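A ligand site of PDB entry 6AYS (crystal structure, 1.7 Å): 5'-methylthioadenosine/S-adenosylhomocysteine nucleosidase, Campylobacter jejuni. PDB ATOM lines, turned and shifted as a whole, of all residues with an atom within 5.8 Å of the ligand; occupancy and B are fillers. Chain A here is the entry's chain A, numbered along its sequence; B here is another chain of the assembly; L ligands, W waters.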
ATOM      1  N   ALA A  18      22.649 -17.396 -30.617  1.00  0.00           N
ATOM      2  CA  ALA A  18      24.079 -17.131 -30.713  1.00  0.00           C
ATOM      3  C   ALA A  18      24.837 -18.245 -31.421  1.00  0.00           C
ATOM      4  O   ALA A  18      25.734 -17.963 -32.210  1.00  0.00           O
ATOM      5  CB  ALA A  18      24.672 -16.921 -29.327  1.00  0.00           C
ATOM      6  N   MET A  19      24.467 -19.494 -31.148  1.00  0.00           N
ATOM      7  CA  MET A  19      25.181 -20.669 -31.687  1.00  0.00           C
ATOM      8  C   MET A  19      24.267 -21.518 -32.535  1.00  0.00           C
ATOM      9  O   MET A  19      23.037 -21.462 -32.407  1.00  0.00           O
ATOM     10  CB  MET A  19      25.735 -21.527 -30.537  1.00  0.00           C
ATOM     11  CG  MET A  19      26.643 -20.787 -29.584  1.00  0.00           C
ATOM     12  SD  MET A  19      27.087 -21.792 -28.153  1.00  0.00           S
ATOM     13  CE  MET A  19      28.070 -23.068 -28.897  1.00  0.00           C
ATOM     14  N   GLU A  22      21.444 -23.462 -30.957  1.00  0.00           N
ATOM     15  CA  GLU A  22      20.262 -22.720 -30.536  1.00  0.00           C
ATOM     16  C   GLU A  22      19.235 -22.474 -31.661  1.00  0.00           C
ATOM     17  O   GLU A  22      18.079 -22.209 -31.374  1.00  0.00           O
ATOM     18  CB  GLU A  22      20.692 -21.387 -29.885  1.00  0.00           C
ATOM     19  CG  GLU A  22      21.521 -21.635 -28.628  1.00  0.00           C
ATOM     20  CD  GLU A  22      22.236 -20.404 -28.090  1.00  0.00           C
ATOM     21  OE1 GLU A  22      22.706 -19.581 -28.901  1.00  0.00           O
ATOM     22  OE2 GLU A  22      22.374 -20.318 -26.849  1.00  0.00           O
ATOM     23  N   ILE A  60      29.078 -15.943 -31.138  1.00  0.00           N
ATOM     24  CA  ILE A  60      29.029 -15.644 -29.710  1.00  0.00           C
ATOM     25  C   ILE A  60      29.359 -14.197 -29.401  1.00  0.00           C
ATOM     26  O   ILE A  60      30.267 -13.612 -30.008  1.00  0.00           O
ATOM     27  CB  ILE A  60      29.977 -16.598 -28.953  1.00  0.00           C
ATOM     28  CG1 ILE A  60      29.445 -18.033 -29.049  1.00  0.00           C
ATOM     29  CG2 ILE A  60      30.167 -16.181 -27.502  1.00  0.00           C
ATOM     30  CD1 ILE A  60      30.475 -19.092 -28.711  1.00  0.00           C
ATOM     31  N   GLY A  61      28.619 -13.632 -28.455  1.00  0.00           N
ATOM     32  CA  GLY A  61      29.011 -12.387 -27.804  1.00  0.00           C
ATOM     33  C   GLY A  61      28.252 -11.149 -28.230  1.00  0.00           C
ATOM     34  O   GLY A  61      27.382 -11.181 -29.115  1.00  0.00           O
ATOM     35  N   VAL A  86      20.540 -20.533 -24.567  1.00  0.00           N
ATOM     36  CA  VAL A  86      20.832 -21.039 -23.230  1.00  0.00           C
ATOM     37  C   VAL A  86      21.473 -19.966 -22.352  1.00  0.00           C
ATOM     38  O   VAL A  86      21.811 -18.896 -22.844  1.00  0.00           O
ATOM     39  CB  VAL A  86      21.675 -22.334 -23.276  1.00  0.00           C
ATOM     40  CG1 VAL A  86      20.947 -23.406 -24.070  1.00  0.00           C
ATOM     41  CG2 VAL A  86      23.067 -22.109 -23.852  1.00  0.00           C
ATOM     42  N   ALA A  87      21.620 -20.254 -21.066  1.00  0.00           N
ATOM     43  CA  ALA A  87      22.204 -19.311 -20.117  1.00  0.00           C
ATOM     44  C   ALA A  87      22.787 -20.017 -18.903  1.00  0.00           C
ATOM     45  O   ALA A  87      22.497 -21.195 -18.661  1.00  0.00           O
ATOM     46  CB  ALA A  87      21.169 -18.278 -19.686  1.00  0.00           C
ATOM     47  N   GLY A  88      23.607 -19.277 -18.152  1.00  0.00           N
ATOM     48  CA  GLY A  88      24.145 -19.735 -16.878  1.00  0.00           C
ATOM     49  C   GLY A  88      23.258 -19.247 -15.740  1.00  0.00           C
ATOM     50  O   GLY A  88      23.022 -18.047 -15.623  1.00  0.00           O
ATOM     51  N   TYR A 108      27.098  -6.209 -17.647  1.00  0.00           N
ATOM     52  CA  TYR A 108      27.924  -6.163 -16.421  1.00  0.00           C
ATOM     53  C   TYR A 108      29.384  -5.754 -16.663  1.00  0.00           C
ATOM     54  O   TYR A 108      30.088  -5.439 -15.704  1.00  0.00           O
ATOM     55  CB  TYR A 108      27.872  -7.494 -15.638  1.00  0.00           C
ATOM     56  CG  TYR A 108      28.482  -8.678 -16.362  1.00  0.00           C
ATOM     57  CD1 TYR A 108      29.861  -8.829 -16.454  1.00  0.00           C
ATOM     58  CD2 TYR A 108      27.669  -9.639 -16.956  1.00  0.00           C
ATOM     59  CE1 TYR A 108      30.428  -9.900 -17.128  1.00  0.00           C
ATOM     60  CE2 TYR A 108      28.213 -10.732 -17.632  1.00  0.00           C
ATOM     61  CZ  TYR A 108      29.589 -10.863 -17.711  1.00  0.00           C
ATOM     62  OH  TYR A 108      30.132 -11.928 -18.385  1.00  0.00           O
ATOM     63  N   GLY A 158      27.435 -10.129 -20.678  1.00  0.00           N
ATOM     64  CA  GLY A 158      28.802  -9.636 -20.883  1.00  0.00           C
ATOM     65  C   GLY A 158      29.548 -10.606 -21.762  1.00  0.00           C
ATOM     66  O   GLY A 158      29.026 -11.669 -22.088  1.00  0.00           O
ATOM     67  N   GLU A 160      32.137 -12.579 -21.312  1.00  0.00           N
ATOM     68  CA  GLU A 160      32.873 -13.642 -20.655  1.00  0.00           C
ATOM     69  C   GLU A 160      31.955 -14.841 -20.396  1.00  0.00           C
ATOM     70  O   GLU A 160      30.820 -14.665 -19.993  1.00  0.00           O
ATOM     71  CB  GLU A 160      33.443 -13.129 -19.324  1.00  0.00           C
ATOM     72  CG  GLU A 160      34.349 -14.116 -18.617  1.00  0.00           C
ATOM     73  CD  GLU A 160      34.985 -13.608 -17.349  1.00  0.00           C
ATOM     74  OE1 GLU A 160      34.819 -12.438 -16.958  1.00  0.00           O
ATOM     75  OE2 GLU A 160      35.689 -14.439 -16.749  1.00  0.00           O
ATOM     76  N   PHE A 161      32.466 -16.052 -20.615  1.00  0.00           N
ATOM     77  CA  PHE A 161      31.784 -17.254 -20.121  1.00  0.00           C
ATOM     78  C   PHE A 161      32.103 -17.360 -18.635  1.00  0.00           C
ATOM     79  O   PHE A 161      33.263 -17.505 -18.255  1.00  0.00           O
ATOM     80  CB  PHE A 161      32.249 -18.518 -20.840  1.00  0.00           C
ATOM     81  CG  PHE A 161      31.536 -19.760 -20.391  1.00  0.00           C
ATOM     82  CD1 PHE A 161      30.275 -20.059 -20.867  1.00  0.00           C
ATOM     83  CD2 PHE A 161      32.123 -20.615 -19.464  1.00  0.00           C
ATOM     84  CE1 PHE A 161      29.601 -21.197 -20.449  1.00  0.00           C
ATOM     85  CE2 PHE A 161      31.459 -21.760 -19.040  1.00  0.00           C
ATOM     86  CZ  PHE A 161      30.204 -22.037 -19.518  1.00  0.00           C
ATOM     87  N   ILE A 162      31.066 -17.256 -17.798  1.00  0.00           N
ATOM     88  CA  ILE A 162      31.232 -17.211 -16.342  1.00  0.00           C
ATOM     89  C   ILE A 162      31.274 -18.634 -15.806  1.00  0.00           C
ATOM     90  O   ILE A 162      30.343 -19.413 -15.994  1.00  0.00           O
ATOM     91  CB  ILE A 162      30.099 -16.413 -15.675  1.00  0.00           C
ATOM     92  CG1 ILE A 162      30.020 -14.982 -16.239  1.00  0.00           C
ATOM     93  CG2 ILE A 162      30.255 -16.395 -14.162  1.00  0.00           C
ATOM     94  CD1 ILE A 162      31.265 -14.155 -16.068  1.00  0.00           C
ATOM     95  N   CYS A 163      32.373 -18.969 -15.116  1.00  0.00           N
ATOM     96  CA  CYS A 163      32.547 -20.303 -14.544  1.00  0.00           C
ATOM     97  C   CYS A 163      33.381 -20.189 -13.284  1.00  0.00           C
ATOM     98  O   CYS A 163      34.403 -20.878 -13.091  1.00  0.00           O
ATOM     99  CB  CYS A 163      33.193 -21.213 -15.582  1.00  0.00           C
ATOM    100  SG  CYS A 163      34.709 -20.563 -16.294  1.00  0.00           S
ATOM    101  N   CYS A 180      23.127 -15.328 -16.384  1.00  0.00           N
ATOM    102  CA  CYS A 180      24.072 -14.623 -17.252  1.00  0.00           C
ATOM    103  C   CYS A 180      24.145 -15.253 -18.627  1.00  0.00           C
ATOM    104  O   CYS A 180      23.848 -16.431 -18.822  1.00  0.00           O
ATOM    105  CB  CYS A 180      25.462 -14.571 -16.642  1.00  0.00           C
ATOM    106  SG  CYS A 180      26.298 -16.161 -16.508  1.00  0.00           S
ATOM    107  N   GLU A 181      24.556 -14.426 -19.587  1.00  0.00           N
ATOM    108  CA  GLU A 181      24.769 -14.864 -20.956  1.00  0.00           C
ATOM    109  C   GLU A 181      25.567 -13.782 -21.687  1.00  0.00           C
ATOM    110  O   GLU A 181      26.052 -12.858 -21.036  1.00  0.00           O
ATOM    111  CB  GLU A 181      23.454 -15.310 -21.639  1.00  0.00           C
ATOM    112  CG  GLU A 181      22.193 -14.547 -21.269  1.00  0.00           C
ATOM    113  CD  GLU A 181      21.965 -13.324 -22.111  1.00  0.00           C
ATOM    114  OE1 GLU A 181      20.832 -13.167 -22.601  1.00  0.00           O
ATOM    115  OE2 GLU A 181      22.922 -12.533 -22.318  1.00  0.00           O
ATOM    116  N   MET A 182      25.740 -13.900 -23.004  1.00  0.00           N
ATOM    117  CA  MET A 182      26.699 -13.040 -23.702  1.00  0.00           C
ATOM    118  C   MET A 182      26.095 -12.249 -24.856  1.00  0.00           C
ATOM    119  O   MET A 182      26.824 -11.636 -25.634  1.00  0.00           O
ATOM    120  CB  MET A 182      27.884 -13.904 -24.178  1.00  0.00           C
ATOM    121  CG  MET A 182      28.561 -14.687 -23.067  1.00  0.00           C
ATOM    122  SD  MET A 182      29.805 -15.880 -23.570  1.00  0.00           S
ATOM    123  CE  MET A 182      31.111 -14.802 -24.189  1.00  0.00           C
ATOM    124  N   GLU A 183      24.757 -12.221 -24.945  1.00  0.00           N
ATOM    125  CA  GLU A 183      24.055 -11.607 -26.079  1.00  0.00           C
ATOM    126  C   GLU A 183      22.755 -10.846 -25.779  1.00  0.00           C
ATOM    127  O   GLU A 183      22.303 -10.076 -26.630  1.00  0.00           O
ATOM    128  CB  GLU A 183      23.731 -12.668 -27.132  1.00  0.00           C
ATOM    129  CG  GLU A 183      24.911 -13.469 -27.677  1.00  0.00           C
ATOM    130  CD  GLU A 183      25.352 -14.645 -26.818  1.00  0.00           C
ATOM    131  OE1 GLU A 183      24.623 -15.088 -25.896  1.00  0.00           O
ATOM    132  OE2 GLU A 183      26.477 -15.142 -27.086  1.00  0.00           O
ATOM    133  N   ARG A 202      15.751 -17.740 -22.319  1.00  0.00           N
ATOM    134  CA  ARG A 202      16.925 -18.580 -22.096  1.00  0.00           C
ATOM    135  C   ARG A 202      16.541 -19.830 -21.311  1.00  0.00           C
ATOM    136  O   ARG A 202      15.800 -19.752 -20.335  1.00  0.00           O
ATOM    137  CB  ARG A 202      17.994 -17.799 -21.333  1.00  0.00           C
ATOM    138  CG  ARG A 202      18.517 -16.538 -22.014  1.00  0.00           C
ATOM    139  CD  ARG A 202      19.289 -16.856 -23.286  1.00  0.00           C
ATOM    140  NE  ARG A 202      20.143 -15.740 -23.742  1.00  0.00           N
ATOM    141  CZ  ARG A 202      21.256 -15.864 -24.483  1.00  0.00           C
ATOM    142  NH1 ARG A 202      21.705 -17.047 -24.870  1.00  0.00           N
ATOM    143  NH2 ARG A 202      21.938 -14.781 -24.842  1.00  0.00           N
ATOM    144  N   SER A 205      21.657 -23.936 -19.110  1.00  0.00           N
ATOM    145  CA  SER A 205      22.585 -25.015 -19.496  1.00  0.00           C
ATOM    146  C   SER A 205      23.586 -25.380 -18.401  1.00  0.00           C
ATOM    147  O   SER A 205      24.229 -26.411 -18.491  1.00  0.00           O
ATOM    148  CB  SER A 205      23.345 -24.624 -20.743  1.00  0.00           C
ATOM    149  OG  SER A 205      24.042 -23.410 -20.550  1.00  0.00           O
ATOM    150  N   ASP A 206      23.731 -24.517 -17.393  1.00  0.00           N
ATOM    151  CA  ASP A 206      24.745 -24.676 -16.365  1.00  0.00           C
ATOM    152  C   ASP A 206      24.464 -23.668 -15.253  1.00  0.00           C
ATOM    153  O   ASP A 206      23.553 -22.852 -15.377  1.00  0.00           O
ATOM    154  CB  ASP A 206      26.151 -24.464 -16.949  1.00  0.00           C
ATOM    155  CG  ASP A 206      26.311 -23.088 -17.547  1.00  0.00           C
ATOM    156  OD1 ASP A 206      26.696 -22.165 -16.807  1.00  0.00           O
ATOM    157  OD2 ASP A 206      26.053 -22.927 -18.760  1.00  0.00           O
ATOM    158  N   LYS A 207      25.247 -23.737 -14.182  1.00  0.00           N
ATOM    159  CA  LYS A 207      25.084 -22.849 -13.022  1.00  0.00           C
ATOM    160  C   LYS A 207      26.232 -21.851 -12.839  1.00  0.00           C
ATOM    161  O   LYS A 207      26.386 -21.264 -11.766  1.00  0.00           O
ATOM    162  CB  LYS A 207      24.896 -23.701 -11.758  1.00  0.00           C
ATOM    163  CG  LYS A 207      23.640 -24.539 -11.815  1.00  0.00           C
ATOM    164  CD  LYS A 207      23.276 -25.152 -10.476  1.00  0.00           C
ATOM    165  CE  LYS A 207      21.921 -25.829 -10.564  1.00  0.00           C
ATOM    166  NZ  LYS A 207      21.446 -26.324  -9.255  1.00  0.00           N
ATOM    167  N   ALA A 208      27.037 -21.662 -13.891  1.00  0.00           N
ATOM    168  CA  ALA A 208      28.019 -20.583 -13.978  1.00  0.00           C
ATOM    169  C   ALA A 208      29.100 -20.553 -12.880  1.00  0.00           C
ATOM    170  O   ALA A 208      29.666 -19.497 -12.596  1.00  0.00           O
ATOM    171  CB  ALA A 208      27.304 -19.241 -14.053  1.00  0.00           C
ATOM    172  N   ALA A 212      31.118 -25.271 -14.814  1.00  0.00           N
ATOM    173  CA  ALA A 212      30.109 -24.736 -15.749  1.00  0.00           C
ATOM    174  C   ALA A 212      30.399 -25.114 -17.193  1.00  0.00           C
ATOM    175  O   ALA A 212      29.478 -25.410 -17.954  1.00  0.00           O
ATOM    176  CB  ALA A 212      29.976 -23.234 -15.613  1.00  0.00           C
ATOM    177  N   PHE A 216      27.718 -27.023 -19.391  1.00  0.00           N
ATOM    178  CA  PHE A 216      27.347 -26.413 -20.674  1.00  0.00           C
ATOM    179  C   PHE A 216      27.505 -27.424 -21.819  1.00  0.00           C
ATOM    180  O   PHE A 216      26.595 -27.572 -22.629  1.00  0.00           O
ATOM    181  CB  PHE A 216      28.174 -25.151 -20.965  1.00  0.00           C
ATOM    182  CG  PHE A 216      27.981 -24.635 -22.357  1.00  0.00           C
ATOM    183  CD1 PHE A 216      26.908 -23.809 -22.671  1.00  0.00           C
ATOM    184  CD2 PHE A 216      28.858 -25.015 -23.372  1.00  0.00           C
ATOM    185  CE1 PHE A 216      26.723 -23.365 -23.973  1.00  0.00           C
ATOM    186  CE2 PHE A 216      28.673 -24.571 -24.674  1.00  0.00           C
ATOM    187  CZ  PHE A 216      27.614 -23.738 -24.972  1.00  0.00           C
ATOM    188  N   ILE B 112      36.142 -16.612 -23.990  1.00  0.00           N
ATOM    189  CA  ILE B 112      35.648 -17.986 -23.813  1.00  0.00           C
ATOM    190  C   ILE B 112      36.824 -18.907 -23.498  1.00  0.00           C
ATOM    191  O   ILE B 112      36.821 -20.080 -23.868  1.00  0.00           O
ATOM    192  CB  ILE B 112      34.831 -18.481 -25.032  1.00  0.00           C
ATOM    193  CG1 ILE B 112      35.649 -18.475 -26.322  1.00  0.00           C
ATOM    194  CG2 ILE B 112      33.574 -17.651 -25.197  1.00  0.00           C
ATOM    195  CD1 ILE B 112      35.055 -19.347 -27.416  1.00  0.00           C
ATOM    196  N   PHE B 115      36.917 -22.650 -22.340  1.00  0.00           N
ATOM    197  CA  PHE B 115      36.871 -23.747 -23.301  1.00  0.00           C
ATOM    198  C   PHE B 115      38.215 -24.009 -24.023  1.00  0.00           C
ATOM    199  O   PHE B 115      38.238 -24.734 -25.042  1.00  0.00           O
ATOM    200  CB  PHE B 115      35.745 -23.482 -24.313  1.00  0.00           C
ATOM    201  CG  PHE B 115      34.383 -23.482 -23.690  1.00  0.00           C
ATOM    202  CD1 PHE B 115      33.682 -24.685 -23.485  1.00  0.00           C
ATOM    203  CD2 PHE B 115      33.807 -22.303 -23.257  1.00  0.00           C
ATOM    204  CE1 PHE B 115      32.449 -24.689 -22.886  1.00  0.00           C
ATOM    205  CE2 PHE B 115      32.542 -22.300 -22.677  1.00  0.00           C
ATOM    206  CZ  PHE B 115      31.867 -23.487 -22.482  1.00  0.00           C
ATOM    207  N   HIS B 117      40.166 -21.844 -25.732  1.00  0.00           N
ATOM    208  CA  HIS B 117      40.516 -20.971 -26.836  1.00  0.00           C
ATOM    209  C   HIS B 117      41.258 -19.733 -26.343  1.00  0.00           C
ATOM    210  O   HIS B 117      41.140 -19.385 -25.166  1.00  0.00           O
ATOM    211  CB  HIS B 117      39.281 -20.588 -27.648  1.00  0.00           C
ATOM    212  CG  HIS B 117      38.731 -21.722 -28.440  1.00  0.00           C
ATOM    213  ND1 HIS B 117      39.364 -22.218 -29.574  1.00  0.00           N
ATOM    214  CD2 HIS B 117      37.609 -22.466 -28.297  1.00  0.00           C
ATOM    215  CE1 HIS B 117      38.652 -23.196 -30.083  1.00  0.00           C
ATOM    216  NE2 HIS B 117      37.566 -23.355 -29.343  1.00  0.00           N
ATOM    217  N   PRO B 123      34.438 -18.890 -32.148  1.00  0.00           N
ATOM    218  CA  PRO B 123      34.360 -19.663 -33.390  1.00  0.00           C
ATOM    219  C   PRO B 123      33.703 -18.918 -34.534  1.00  0.00           C
ATOM    220  O   PRO B 123      32.704 -18.211 -34.319  1.00  0.00           O
ATOM    221  CB  PRO B 123      33.517 -20.885 -33.001  1.00  0.00           C
ATOM    222  CG  PRO B 123      33.763 -21.049 -31.552  1.00  0.00           C
ATOM    223  CD  PRO B 123      33.911 -19.664 -31.001  1.00  0.00           C
HETATM  224  O1  LIG L   1      26.880 -17.838 -26.716  1.00  0.00           O
HETATM  225  C1  LIG L   1      27.517 -18.048 -25.447  1.00  0.00           C
HETATM  226  C2  LIG L   1      27.672 -19.521 -25.140  1.00  0.00           C
HETATM  227  C3  LIG L   1      28.805 -19.793 -24.131  1.00  0.00           C
HETATM  228  S1  LIG L   1      30.416 -19.664 -24.847  1.00  0.00           S
HETATM  229  C4  LIG L   1      30.557 -21.203 -25.693  1.00  0.00           C
HETATM  230  C5  LIG L   1      31.939 -21.450 -26.255  1.00  0.00           C
HETATM  231  C6  LIG L   1      32.084 -22.931 -26.605  1.00  0.00           C
HETATM  232  C7  LIG L   1      33.442 -23.221 -27.248  1.00  0.00           C
HETATM  233  C8  LIG L   1      33.676 -24.723 -27.331  1.00  0.00           C
HETATM  234  C9  LIG L   1      35.021 -25.051 -27.960  1.00  0.00           C
HETATM  235  C10 LIG L   1      26.640 -17.549 -24.335  1.00  0.00           C
HETATM  236  N1  LIG L   1      25.654 -18.631 -24.223  1.00  0.00           N
HETATM  237  C11 LIG L   1      26.314 -19.915 -24.559  1.00  0.00           C
HETATM  238  C12 LIG L   1      24.908 -18.602 -22.973  1.00  0.00           C
HETATM  239  C13 LIG L   1      25.576 -19.115 -21.718  1.00  0.00           C
HETATM  240  C14 LIG L   1      26.573 -18.460 -20.865  1.00  0.00           C
HETATM  241  N2  LIG L   1      27.211 -17.270 -20.967  1.00  0.00           N
HETATM  242  C15 LIG L   1      28.085 -16.915 -20.037  1.00  0.00           C
HETATM  243  N3  LIG L   1      28.409 -17.711 -18.988  1.00  0.00           N
HETATM  244  C16 LIG L   1      27.819 -18.895 -18.776  1.00  0.00           C
HETATM  245  N4  LIG L   1      28.149 -19.650 -17.705  1.00  0.00           N
HETATM  246  C17 LIG L   1      26.831 -19.372 -19.763  1.00  0.00           C
HETATM  247  N5  LIG L   1      26.067 -20.450 -19.937  1.00  0.00           N
HETATM  248  C18 LIG L   1      25.311 -20.316 -21.071  1.00  0.00           C
HETATM  249  O   HOH W   1      28.234 -13.584 -19.388  1.00  0.00           O
HETATM  250  O   HOH W   2      23.906 -18.205 -26.219  1.00  0.00           O
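Ala 18 touches the ligand (CB to O1, 3.5 Å).
Met 19 touches the ligand.
Ile 60 touches the ligand (CG1 to O1, 3.5 Å).
Val 86 touches the ligand (O to C12, 3.1 Å).
Ala 87 touches the ligand (C to C18, 3.3 Å).
Glu 160 touches the ligand (O to C15, 3.5 Å).
Phe 161 touches the ligand (CE1 to C16, 3.4 Å).
Glu 181 touches the ligand.
CG of Met 182 touches N2 of the ligand, at 3.6 Å.
OG of Ser 205 touches C18 of the ligand, at 3.4 Å.
CB of Ala 208 touches N4 of the ligand (3.8 Å).
Phe 216 touches the ligand (CE1 to C11, 3.5 Å).
Ile 112 of chain B touches the ligand.
Phe 115 of chain B touches the ligand (CD2 to C5, 3.6 Å).
His 117 of chain B touches the ligand.
Hydrophobic or aromatic side chains within 4 Å of the ligand: Ala 18, Met 19, Ile 60, Val 86, Phe 161, Ile 162, Met 182, Ala 208, Phe 216, Ile 112 of chain B, Phe 115 of chain B and His 117 of chain B.
20 residues have an atom within 4 Å of the ligand: Ala 18, Met 19, Ile 60, Val 86, Ala 87, Gly 88, Glu 160, Phe 161, Ile 162, Cys 180, Glu 181, Met 182, Glu 183, Ser 205, Asp 206, Ala 208, Phe 216, Ile 112 of chain B, Phe 115 of chain B and His 117 of chain B.
The backbone carbonyl oxygen (O) of Ile 162 is in hydrogen-bond range of a nitrogen (N4) of the ligand.
OD2 of Asp 206 lies within hydrogen-bond range of N5 of the ligand (2.7 Å).
A nitrogen (N3) of the ligand lies within hydrogen-bond range of the side-chain sulfur (SG) of Cys 180, at 3.6 Å.
N of Gly 88 lies close to N5 of the ligand.
The side-chain carboxylate of Glu 183 sits at hydrogen-bond distance from an oxygen (O1) of the ligand, at 2.8 Å.
The backbone NH of Ile 162 sits at hydrogen-bond distance from a nitrogen (N3) of the ligand, at 2.9 Å.
Water W2 lies within hydrogen-bond range of OE2 of Glu 22 (2.7 Å), NH1 of Arg 202 (2.8 Å), O1 of the ligand (3.0 Å) and OE1 of Glu 183 (3.2 Å).
NH1 of Arg 202 lies within hydrogen-bond range of O of Val 86, at 2.7 Å.
The side-chain carboxylate of Glu 183 is in salt-bridge range of the guanidinium group of Arg 202, at 2.9 Å.
The side-chain carboxylate of Asp 206 lies within hydrogen-bond range of the side-chain hydroxyl of Ser 205, at 2.7 Å.
The side-chain carboxylate (OE1) of Glu 181 is in salt-bridge range of the guanidinium group (NE) of Arg 202, 2.9 Å away.
The side-chain carboxylate of Glu 22 lies within hydrogen-bond range of the backbone NH of Val 86 (2.9 Å).
The backbone NH (N) of Ala 208 lies within hydrogen-bond range of the side-chain carboxylate (OD1) of Asp 206, 3.0 Å away.
The backbone carbonyl oxygen (O) of Glu 181 lies within hydrogen-bond range of the backbone NH (N) of Gly 158, at 3.1 Å.
The backbone NH (N) of Ser 205 is in hydrogen-bond range of the backbone carbonyl oxygen (O) of Ala 87 (2.9 Å).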
